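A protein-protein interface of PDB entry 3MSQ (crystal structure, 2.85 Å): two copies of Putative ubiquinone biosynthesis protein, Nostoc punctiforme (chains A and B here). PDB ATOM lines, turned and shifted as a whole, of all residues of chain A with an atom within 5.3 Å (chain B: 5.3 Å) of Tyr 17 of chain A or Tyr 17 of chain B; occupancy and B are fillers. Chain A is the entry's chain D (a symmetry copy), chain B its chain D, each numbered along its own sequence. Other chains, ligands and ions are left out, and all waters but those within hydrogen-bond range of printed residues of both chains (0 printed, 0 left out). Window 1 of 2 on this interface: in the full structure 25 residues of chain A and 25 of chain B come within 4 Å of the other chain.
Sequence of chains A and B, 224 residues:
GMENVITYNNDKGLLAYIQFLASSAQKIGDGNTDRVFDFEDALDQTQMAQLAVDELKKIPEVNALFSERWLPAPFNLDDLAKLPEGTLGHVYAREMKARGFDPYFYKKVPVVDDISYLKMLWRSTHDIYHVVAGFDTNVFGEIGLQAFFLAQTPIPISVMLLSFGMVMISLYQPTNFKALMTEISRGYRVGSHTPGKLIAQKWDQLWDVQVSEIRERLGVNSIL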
ATOM      1  N   LYS A  12      11.805   4.504  26.225  1.00  0.00           N
ATOM      2  CA  LYS A  12      12.194   3.224  26.804  1.00  0.00           C
ATOM      3  C   LYS A  12      11.474   2.065  26.114  1.00  0.00           C
ATOM      4  O   LYS A  12      12.022   0.969  26.036  1.00  0.00           O
ATOM      5  CB  LYS A  12      12.032   3.214  28.322  1.00  0.00           C
ATOM      6  CG  LYS A  12      13.118   4.027  29.035  1.00  0.00           C
ATOM      7  CD  LYS A  12      13.204   3.702  30.516  1.00  0.00           C
ATOM      8  CE  LYS A  12      14.059   4.676  31.280  1.00  0.00           C
ATOM      9  NZ  LYS A  12      15.504   4.571  30.929  1.00  0.00           N
ATOM     10  N   GLY A  13      10.302   2.340  25.549  1.00  0.00           N
ATOM     11  CA  GLY A  13       9.549   1.382  24.752  1.00  0.00           C
ATOM     12  C   GLY A  13      10.311   1.107  23.463  1.00  0.00           C
ATOM     13  O   GLY A  13      10.489  -0.054  23.092  1.00  0.00           O
ATOM     14  N   LEU A  14      10.833   2.175  22.804  1.00  0.00           N
ATOM     15  CA  LEU A  14      11.643   2.058  21.581  1.00  0.00           C
ATOM     16  C   LEU A  14      12.947   1.300  21.863  1.00  0.00           C
ATOM     17  O   LEU A  14      13.363   0.463  21.050  1.00  0.00           O
ATOM     18  CB  LEU A  14      11.945   3.443  20.961  1.00  0.00           C
ATOM     19  CG  LEU A  14      12.730   3.436  19.642  1.00  0.00           C
ATOM     20  CD1 LEU A  14      12.060   2.552  18.623  1.00  0.00           C
ATOM     21  CD2 LEU A  14      12.949   4.837  19.114  1.00  0.00           C
ATOM     22  N   LEU A  15      13.579   1.587  23.013  1.00  0.00           N
ATOM     23  CA  LEU A  15      14.798   0.904  23.425  1.00  0.00           C
ATOM     24  C   LEU A  15      14.532  -0.586  23.633  1.00  0.00           C
ATOM     25  O   LEU A  15      15.357  -1.405  23.239  1.00  0.00           O
ATOM     26  CB  LEU A  15      15.387   1.540  24.688  1.00  0.00           C
ATOM     27  CG  LEU A  15      16.105   2.874  24.477  1.00  0.00           C
ATOM     28  CD1 LEU A  15      16.293   3.625  25.796  1.00  0.00           C
ATOM     29  CD2 LEU A  15      17.446   2.692  23.719  1.00  0.00           C
ATOM     30  N   ALA A  16      13.348  -0.931  24.181  1.00  0.00           N
ATOM     31  CA  ALA A  16      12.920  -2.305  24.422  1.00  0.00           C
ATOM     32  C   ALA A  16      12.705  -3.076  23.107  1.00  0.00           C
ATOM     33  O   ALA A  16      13.013  -4.276  23.038  1.00  0.00           O
ATOM     34  CB  ALA A  16      11.652  -2.306  25.241  1.00  0.00           C
ATOM     35  N   TYR A  17      12.179  -2.386  22.074  1.00  0.00           N
ATOM     36  CA  TYR A  17      11.927  -2.934  20.745  1.00  0.00           C
ATOM     37  C   TYR A  17      13.257  -3.183  20.022  1.00  0.00           C
ATOM     38  O   TYR A  17      13.436  -4.237  19.414  1.00  0.00           O
ATOM     39  CB  TYR A  17      11.005  -1.981  19.958  1.00  0.00           C
ATOM     40  CG  TYR A  17      10.697  -2.403  18.537  1.00  0.00           C
ATOM     41  CD1 TYR A  17       9.992  -3.575  18.270  1.00  0.00           C
ATOM     42  CD2 TYR A  17      11.051  -1.598  17.459  1.00  0.00           C
ATOM     43  CE1 TYR A  17       9.679  -3.950  16.964  1.00  0.00           C
ATOM     44  CE2 TYR A  17      10.751  -1.969  16.148  1.00  0.00           C
ATOM     45  CZ  TYR A  17      10.059  -3.138  15.907  1.00  0.00           C
ATOM     46  OH  TYR A  17       9.757  -3.468  14.618  1.00  0.00           O
ATOM     47  N   ILE A  18      14.201  -2.222  20.126  1.00  0.00           N
ATOM     48  CA  ILE A  18      15.537  -2.326  19.549  1.00  0.00           C
ATOM     49  C   ILE A  18      16.257  -3.527  20.208  1.00  0.00           C
ATOM     50  O   ILE A  18      16.895  -4.324  19.507  1.00  0.00           O
ATOM     51  CB  ILE A  18      16.300  -0.967  19.690  1.00  0.00           C
ATOM     52  CG1 ILE A  18      15.770   0.063  18.660  1.00  0.00           C
ATOM     53  CG2 ILE A  18      17.831  -1.142  19.574  1.00  0.00           C
ATOM     54  CD1 ILE A  18      16.163   1.498  18.865  1.00  0.00           C
ATOM     55  N   GLN A  19      16.099  -3.674  21.544  1.00  0.00           N
ATOM     56  CA  GLN A  19      16.668  -4.776  22.322  1.00  0.00           C
ATOM     57  C   GLN A  19      16.131  -6.102  21.770  1.00  0.00           C
ATOM     58  O   GLN A  19      16.920  -6.992  21.433  1.00  0.00           O
ATOM     59  CB  GLN A  19      16.314  -4.607  23.807  1.00  0.00           C
ATOM     60  CG  GLN A  19      16.823  -5.710  24.724  1.00  0.00           C
ATOM     61  CD  GLN A  19      16.159  -5.705  26.083  1.00  0.00           C
ATOM     62  OE1 GLN A  19      15.671  -4.688  26.589  1.00  0.00           O
ATOM     63  NE2 GLN A  19      16.180  -6.845  26.742  1.00  0.00           N
ATOM     64  N   PHE A  20      14.789  -6.184  21.614  1.00  0.00           N
ATOM     65  CA  PHE A  20      14.070  -7.335  21.102  1.00  0.00           C
ATOM     66  C   PHE A  20      14.514  -7.737  19.680  1.00  0.00           C
ATOM     67  O   PHE A  20      14.827  -8.915  19.447  1.00  0.00           O
ATOM     68  CB  PHE A  20      12.555  -7.094  21.174  1.00  0.00           C
ATOM     69  CG  PHE A  20      11.718  -8.343  21.012  1.00  0.00           C
ATOM     70  CD1 PHE A  20      11.828  -9.394  21.915  1.00  0.00           C
ATOM     71  CD2 PHE A  20      10.807  -8.459  19.973  1.00  0.00           C
ATOM     72  CE1 PHE A  20      11.090 -10.564  21.743  1.00  0.00           C
ATOM     73  CE2 PHE A  20      10.046  -9.621  19.818  1.00  0.00           C
ATOM     74  CZ  PHE A  20      10.198 -10.670  20.699  1.00  0.00           C
ATOM     75  N   LEU A  21      14.598  -6.762  18.750  1.00  0.00           N
ATOM     76  CA  LEU A  21      15.046  -7.025  17.380  1.00  0.00           C
ATOM     77  C   LEU A  21      16.448  -7.612  17.381  1.00  0.00           C
ATOM     78  O   LEU A  21      16.684  -8.630  16.735  1.00  0.00           O
ATOM     79  CB  LEU A  21      15.049  -5.736  16.539  1.00  0.00           C
ATOM     80  CG  LEU A  21      13.718  -5.051  16.257  1.00  0.00           C
ATOM     81  CD1 LEU A  21      13.940  -3.605  15.915  1.00  0.00           C
ATOM     82  CD2 LEU A  21      12.922  -5.738  15.169  1.00  0.00           C
ATOM     83  N   ALA A  22      17.367  -6.971  18.128  1.00  0.00           N
ATOM     84  CA  ALA A  22      18.784  -7.329  18.218  1.00  0.00           C
ATOM     85  C   ALA A  22      19.044  -8.680  18.877  1.00  0.00           C
ATOM     86  O   ALA A  22      19.901  -9.406  18.385  1.00  0.00           O
ATOM     87  CB  ALA A  22      19.571  -6.221  18.902  1.00  0.00           C
ATOM     88  N   PHE A  39      10.252  -7.812  27.288  1.00  0.00           N
ATOM     89  CA  PHE A  39       9.786  -6.788  26.351  1.00  0.00           C
ATOM     90  C   PHE A  39       8.419  -6.254  26.783  1.00  0.00           C
ATOM     91  O   PHE A  39       8.243  -5.039  26.908  1.00  0.00           O
ATOM     92  CB  PHE A  39       9.738  -7.356  24.917  1.00  0.00           C
ATOM     93  CG  PHE A  39       9.378  -6.403  23.799  1.00  0.00           C
ATOM     94  CD1 PHE A  39       9.543  -5.028  23.947  1.00  0.00           C
ATOM     95  CD2 PHE A  39       8.927  -6.881  22.578  1.00  0.00           C
ATOM     96  CE1 PHE A  39       9.196  -4.152  22.918  1.00  0.00           C
ATOM     97  CE2 PHE A  39       8.608  -6.002  21.543  1.00  0.00           C
ATOM     98  CZ  PHE A  39       8.745  -4.646  21.719  1.00  0.00           C
ATOM     99  N   MET A 160       3.843  -4.567  18.420  1.00  0.00           N
ATOM    100  CA  MET A 160       5.287  -4.794  18.449  1.00  0.00           C
ATOM    101  C   MET A 160       5.633  -6.122  17.783  1.00  0.00           C
ATOM    102  O   MET A 160       6.474  -6.137  16.887  1.00  0.00           O
ATOM    103  CB  MET A 160       5.825  -4.733  19.882  1.00  0.00           C
ATOM    104  CG  MET A 160       5.620  -3.368  20.581  1.00  0.00           C
ATOM    105  SD  MET A 160       6.348  -1.819  19.626  1.00  0.00           S
ATOM    106  CE  MET A 160       4.722  -1.029  19.194  1.00  0.00           C
ATOM    107  N   SER A 163       5.068  -5.961  13.776  1.00  0.00           N
ATOM    108  CA  SER A 163       6.187  -5.224  13.150  1.00  0.00           C
ATOM    109  C   SER A 163       7.444  -6.075  13.140  1.00  0.00           C
ATOM    110  O   SER A 163       8.074  -6.249  12.091  1.00  0.00           O
ATOM    111  CB  SER A 163       6.471  -3.932  13.898  1.00  0.00           C
ATOM    112  OG  SER A 163       5.369  -3.047  13.801  1.00  0.00           O
ATOM    113  N   PHE A 164       7.772  -6.648  14.312  1.00  0.00           N
ATOM    114  CA  PHE A 164       8.902  -7.542  14.530  1.00  0.00           C
ATOM    115  C   PHE A 164       8.862  -8.697  13.523  1.00  0.00           C
ATOM    116  O   PHE A 164       9.851  -8.931  12.825  1.00  0.00           O
ATOM    117  CB  PHE A 164       8.871  -8.067  15.977  1.00  0.00           C
ATOM    118  CG  PHE A 164       9.835  -9.182  16.253  1.00  0.00           C
ATOM    119  CD1 PHE A 164      11.164  -8.910  16.553  1.00  0.00           C
ATOM    120  CD2 PHE A 164       9.422 -10.508  16.198  1.00  0.00           C
ATOM    121  CE1 PHE A 164      12.056  -9.945  16.822  1.00  0.00           C
ATOM    122  CE2 PHE A 164      10.316 -11.539  16.446  1.00  0.00           C
ATOM    123  CZ  PHE A 164      11.627 -11.255  16.748  1.00  0.00           C
ATOM    124  N   VAL A 167       9.546  -7.570   9.862  1.00  0.00           N
ATOM    125  CA  VAL A 167      10.966  -7.191   9.752  1.00  0.00           C
ATOM    126  C   VAL A 167      11.900  -8.413   9.759  1.00  0.00           C
ATOM    127  O   VAL A 167      12.773  -8.519   8.894  1.00  0.00           O
ATOM    128  CB  VAL A 167      11.329  -6.178  10.862  1.00  0.00           C
ATOM    129  CG1 VAL A 167      12.823  -5.917  10.910  1.00  0.00           C
ATOM    130  CG2 VAL A 167      10.572  -4.868  10.673  1.00  0.00           C
ATOM    131  N   LYS B  12      23.115  -6.080   8.337  1.00  0.00           N
ATOM    132  CA  LYS B  12      23.281  -4.665   8.029  1.00  0.00           C
ATOM    133  C   LYS B  12      21.938  -4.008   7.712  1.00  0.00           C
ATOM    134  O   LYS B  12      21.764  -2.820   7.973  1.00  0.00           O
ATOM    135  CB  LYS B  12      24.332  -4.439   6.945  1.00  0.00           C
ATOM    136  CG  LYS B  12      25.761  -4.640   7.461  1.00  0.00           C
ATOM    137  CD  LYS B  12      26.801  -4.041   6.529  1.00  0.00           C
ATOM    138  CE  LYS B  12      28.203  -4.466   6.868  1.00  0.00           C
ATOM    139  NZ  LYS B  12      28.682  -3.893   8.158  1.00  0.00           N
ATOM    140  N   GLY B  13      20.981  -4.801   7.237  1.00  0.00           N
ATOM    141  CA  GLY B  13      19.614  -4.359   7.000  1.00  0.00           C
ATOM    142  C   GLY B  13      18.954  -4.059   8.338  1.00  0.00           C
ATOM    143  O   GLY B  13      18.335  -3.005   8.494  1.00  0.00           O
ATOM    144  N   LEU B  14      19.140  -4.955   9.343  1.00  0.00           N
ATOM    145  CA  LEU B  14      18.614  -4.769  10.705  1.00  0.00           C
ATOM    146  C   LEU B  14      19.248  -3.539  11.369  1.00  0.00           C
ATOM    147  O   LEU B  14      18.548  -2.771  12.043  1.00  0.00           O
ATOM    148  CB  LEU B  14      18.831  -6.028  11.578  1.00  0.00           C
ATOM    149  CG  LEU B  14      18.261  -5.968  13.002  1.00  0.00           C
ATOM    150  CD1 LEU B  14      16.800  -5.602  12.980  1.00  0.00           C
ATOM    151  CD2 LEU B  14      18.507  -7.256  13.757  1.00  0.00           C
ATOM    152  N   LEU B  15      20.564  -3.353  11.170  1.00  0.00           N
ATOM    153  CA  LEU B  15      21.277  -2.199  11.701  1.00  0.00           C
ATOM    154  C   LEU B  15      20.731  -0.907  11.097  1.00  0.00           C
ATOM    155  O   LEU B  15      20.574   0.075  11.817  1.00  0.00           O
ATOM    156  CB  LEU B  15      22.785  -2.325  11.462  1.00  0.00           C
ATOM    157  CG  LEU B  15      23.515  -3.307  12.381  1.00  0.00           C
ATOM    158  CD1 LEU B  15      24.891  -3.676  11.825  1.00  0.00           C
ATOM    159  CD2 LEU B  15      23.602  -2.777  13.835  1.00  0.00           C
ATOM    160  N   ALA B  16      20.373  -0.937   9.796  1.00  0.00           N
ATOM    161  CA  ALA B  16      19.808   0.196   9.070  1.00  0.00           C
ATOM    162  C   ALA B  16      18.412   0.575   9.599  1.00  0.00           C
ATOM    163  O   ALA B  16      18.077   1.768   9.654  1.00  0.00           O
ATOM    164  CB  ALA B  16      19.738  -0.129   7.597  1.00  0.00           C
ATOM    165  N   TYR B  17      17.609  -0.438   9.983  1.00  0.00           N
ATOM    166  CA  TYR B  17      16.267  -0.279  10.533  1.00  0.00           C
ATOM    167  C   TYR B  17      16.349   0.314  11.946  1.00  0.00           C
ATOM    168  O   TYR B  17      15.594   1.228  12.272  1.00  0.00           O
ATOM    169  CB  TYR B  17      15.533  -1.634  10.512  1.00  0.00           C
ATOM    170  CG  TYR B  17      14.139  -1.627  11.102  1.00  0.00           C
ATOM    171  CD1 TYR B  17      13.116  -0.875  10.525  1.00  0.00           C
ATOM    172  CD2 TYR B  17      13.821  -2.423  12.197  1.00  0.00           C
ATOM    173  CE1 TYR B  17      11.824  -0.891  11.047  1.00  0.00           C
ATOM    174  CE2 TYR B  17      12.533  -2.439  12.733  1.00  0.00           C
ATOM    175  CZ  TYR B  17      11.539  -1.680  12.150  1.00  0.00           C
ATOM    176  OH  TYR B  17      10.281  -1.729  12.678  1.00  0.00           O
ATOM    177  N   ILE B  18      17.299  -0.186  12.766  1.00  0.00           N
ATOM    178  CA  ILE B  18      17.549   0.304  14.118  1.00  0.00           C
ATOM    179  C   ILE B  18      17.984   1.786  14.022  1.00  0.00           C
ATOM    180  O   ILE B  18      17.504   2.622  14.801  1.00  0.00           O
ATOM    181  CB  ILE B  18      18.578  -0.620  14.852  1.00  0.00           C
ATOM    182  CG1 ILE B  18      17.902  -1.943  15.293  1.00  0.00           C
ATOM    183  CG2 ILE B  18      19.254   0.092  16.045  1.00  0.00           C
ATOM    184  CD1 ILE B  18      18.807  -3.062  15.721  1.00  0.00           C
ATOM    185  N   GLN B  19      18.849   2.105  13.032  1.00  0.00           N
ATOM    186  CA  GLN B  19      19.330   3.462  12.766  1.00  0.00           C
ATOM    187  C   GLN B  19      18.126   4.365  12.469  1.00  0.00           C
ATOM    188  O   GLN B  19      17.965   5.408  13.113  1.00  0.00           O
ATOM    189  CB  GLN B  19      20.319   3.447  11.592  1.00  0.00           C
ATOM    190  CG  GLN B  19      20.871   4.808  11.193  1.00  0.00           C
ATOM    191  CD  GLN B  19      21.536   4.804   9.834  1.00  0.00           C
ATOM    192  OE1 GLN B  19      22.034   3.789   9.333  1.00  0.00           O
ATOM    193  NE2 GLN B  19      21.616   5.968   9.225  1.00  0.00           N
ATOM    194  N   PHE B  20      17.252   3.907  11.542  1.00  0.00           N
ATOM    195  CA  PHE B  20      16.045   4.590  11.114  1.00  0.00           C
ATOM    196  C   PHE B  20      15.065   4.861  12.275  1.00  0.00           C
ATOM    197  O   PHE B  20      14.617   6.007  12.442  1.00  0.00           O
ATOM    198  CB  PHE B  20      15.369   3.816   9.973  1.00  0.00           C
ATOM    199  CG  PHE B  20      14.327   4.607   9.217  1.00  0.00           C
ATOM    200  CD1 PHE B  20      14.672   5.769   8.536  1.00  0.00           C
ATOM    201  CD2 PHE B  20      13.008   4.181   9.167  1.00  0.00           C
ATOM    202  CE1 PHE B  20      13.704   6.524   7.874  1.00  0.00           C
ATOM    203  CE2 PHE B  20      12.044   4.923   8.479  1.00  0.00           C
ATOM    204  CZ  PHE B  20      12.395   6.094   7.845  1.00  0.00           C
ATOM    205  N   LEU B  21      14.776   3.836  13.104  1.00  0.00           N
ATOM    206  CA  LEU B  21      13.889   3.993  14.260  1.00  0.00           C
ATOM    207  C   LEU B  21      14.429   5.052  15.207  1.00  0.00           C
ATOM    208  O   LEU B  21      13.689   5.947  15.607  1.00  0.00           O
ATOM    209  CB  LEU B  21      13.741   2.668  15.030  1.00  0.00           C
ATOM    210  CG  LEU B  21      13.065   1.495  14.332  1.00  0.00           C
ATOM    211  CD1 LEU B  21      13.470   0.202  14.980  1.00  0.00           C
ATOM    212  CD2 LEU B  21      11.557   1.622  14.295  1.00  0.00           C
ATOM    213  N   ALA B  22      15.729   4.951  15.544  1.00  0.00           N
ATOM    214  CA  ALA B  22      16.428   5.824  16.487  1.00  0.00           C
ATOM    215  C   ALA B  22      16.559   7.270  16.019  1.00  0.00           C
ATOM    216  O   ALA B  22      16.380   8.161  16.842  1.00  0.00           O
ATOM    217  CB  ALA B  22      17.785   5.238  16.850  1.00  0.00           C
ATOM    218  N   PHE B  39      18.455   4.724   4.240  1.00  0.00           N
ATOM    219  CA  PHE B  39      17.882   3.447   4.670  1.00  0.00           C
ATOM    220  C   PHE B  39      17.667   2.528   3.466  1.00  0.00           C
ATOM    221  O   PHE B  39      18.121   1.382   3.477  1.00  0.00           O
ATOM    222  CB  PHE B  39      16.564   3.683   5.437  1.00  0.00           C
ATOM    223  CG  PHE B  39      15.884   2.477   6.048  1.00  0.00           C
ATOM    224  CD1 PHE B  39      16.601   1.317   6.330  1.00  0.00           C
ATOM    225  CD2 PHE B  39      14.543   2.519   6.393  1.00  0.00           C
ATOM    226  CE1 PHE B  39      15.968   0.202   6.880  1.00  0.00           C
ATOM    227  CE2 PHE B  39      13.921   1.410   6.968  1.00  0.00           C
ATOM    228  CZ  PHE B  39      14.636   0.262   7.209  1.00  0.00           C
ATOM    229  N   MET B 160       9.529  -2.252   5.621  1.00  0.00           N
ATOM    230  CA  MET B 160      10.248  -1.499   6.648  1.00  0.00           C
ATOM    231  C   MET B 160       9.435  -0.285   7.086  1.00  0.00           C
ATOM    232  O   MET B 160       9.211  -0.119   8.283  1.00  0.00           O
ATOM    233  CB  MET B 160      11.640  -1.091   6.158  1.00  0.00           C
ATOM    234  CG  MET B 160      12.567  -2.280   5.811  1.00  0.00           C
ATOM    235  SD  MET B 160      12.824  -3.589   7.246  1.00  0.00           S
ATOM    236  CE  MET B 160      11.914  -4.996   6.441  1.00  0.00           C
ATOM    237  N   SER B 163       6.175  -1.376   9.225  1.00  0.00           N
ATOM    238  CA  SER B 163       6.585  -1.741  10.597  1.00  0.00           C
ATOM    239  C   SER B 163       6.939  -0.497  11.395  1.00  0.00           C
ATOM    240  O   SER B 163       6.426  -0.296  12.500  1.00  0.00           O
ATOM    241  CB  SER B 163       7.787  -2.672  10.575  1.00  0.00           C
ATOM    242  OG  SER B 163       7.449  -3.907   9.969  1.00  0.00           O
ATOM    243  N   PHE B 164       7.784   0.360  10.796  1.00  0.00           N
ATOM    244  CA  PHE B 164       8.224   1.637  11.343  1.00  0.00           C
ATOM    245  C   PHE B 164       7.012   2.487  11.740  1.00  0.00           C
ATOM    246  O   PHE B 164       6.934   2.943  12.882  1.00  0.00           O
ATOM    247  CB  PHE B 164       9.100   2.367  10.309  1.00  0.00           C
ATOM    248  CG  PHE B 164       9.412   3.792  10.657  1.00  0.00           C
ATOM    249  CD1 PHE B 164      10.458   4.099  11.517  1.00  0.00           C
ATOM    250  CD2 PHE B 164       8.649   4.832  10.137  1.00  0.00           C
ATOM    251  CE1 PHE B 164      10.755   5.423  11.828  1.00  0.00           C
ATOM    252  CE2 PHE B 164       8.932   6.150  10.465  1.00  0.00           C
ATOM    253  CZ  PHE B 164       9.976   6.438  11.312  1.00  0.00           C
ATOM    254  N   VAL B 167       5.049   1.049  14.776  1.00  0.00           N
ATOM    255  CA  VAL B 167       5.877   1.216  15.984  1.00  0.00           C
ATOM    256  C   VAL B 167       5.930   2.678  16.459  1.00  0.00           C
ATOM    257  O   VAL B 167       5.712   2.944  17.643  1.00  0.00           O
ATOM    258  CB  VAL B 167       7.289   0.635  15.740  1.00  0.00           C
ATOM    259  CG1 VAL B 167       8.232   0.968  16.882  1.00  0.00           C
ATOM    260  CG2 VAL B 167       7.229  -0.874  15.530  1.00  0.00           C
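Of the 16 printed residues of chain B, 5 touch a printed residue of chain A.
Hydrophobic or aromatic side chains of chain B that line the printed part of chain A: Leu 14, Tyr 17, Leu 21 and Val 167.
Of the 16 printed residues of chain A, 5 touch a printed residue of chain B.
Hydrophobic or aromatic side chains of chain A that line the printed part of chain B: Leu 14, Tyr 17, Leu 21 and Val 167.
Along chain A the printed residues that touch a printed residue of chain B span positions 14 to 167.
Among the printed residues, 11 pairs touch across the chains.
Among the printed residues, no Asp or Glu carboxylate lies within 4 Å of a Lys or Arg side-chain nitrogen of the other chain.
O of Ser 163 of chain B is in hydrogen-bond range of OG of Ser 163 of chain A, 3.2 Å away.
The side-chain hydroxyl of Tyr 17 of chain B is in hydrogen-bond range of the side-chain hydroxyl of Tyr 17 of chain A (2.7 Å).
Among the printed residues, merely in contact across the chains: Leu 14 of chain A with Leu 21 of chain B, Tyr 17 of chain A with Leu 21 of chain B, Tyr 17 of chain A with Val 167 of chain B, Leu 21 of chain A with Leu 14 of chain B, Leu 21 of chain A with Tyr 17 of chain B, Leu 21 of chain A with Leu 21 of chain B, Ser 163 of chain A with Val 167 of chain B, Val 167 of chain A with Tyr 17 of chain B and Val 167 of chain A with Ser 163 of chain B.
Tyr 17 of chain A touches Leu 21 of chain B, and with the chains exchanged Leu 21 of chain A touches Tyr 17 of chain B.
Tyr 17 of chain A touches Val 167 of chain B, and with the chains exchanged Val 167 of chain A touches Tyr 17 of chain B.
Ser 163 of chain A touches its own counterpart, Ser 163 of chain B.
Ser 163 of chain A touches Val 167 of chain B, and with the chains exchanged Val 167 of chain A touches Ser 163 of chain B.
Positions printed for both chains: 12, 13, 14, 15, 16, 17, 18, 19, 20, 21, 22, 39, 160, 163, 164 and 167.
Of the 11 pairs that touch across the chains among the printed residues, 11 have their exchanged pair printed and touching as well.
Of chain B, only Tyr 17 (2.7 Å), Leu 21 (3.7 Å) and Val 167 (3.6 Å) come within 4 Å of Tyr 17 of chain A.
Of the printed residues of chain A, Leu 14 of chain B touches Leu 21 (3.8 Å).
Printed residues of chain A within 4 Å of Tyr 17 of chain B: Tyr 17, Leu 21 and Val 167.
Of the printed residues of chain A, Ser 163 of chain B touches Ser 163 and Val 167.
The nearest printed residue of chain A that does not touch Leu 14 of chain B is Ala 22 of chain A (4.5 Å).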
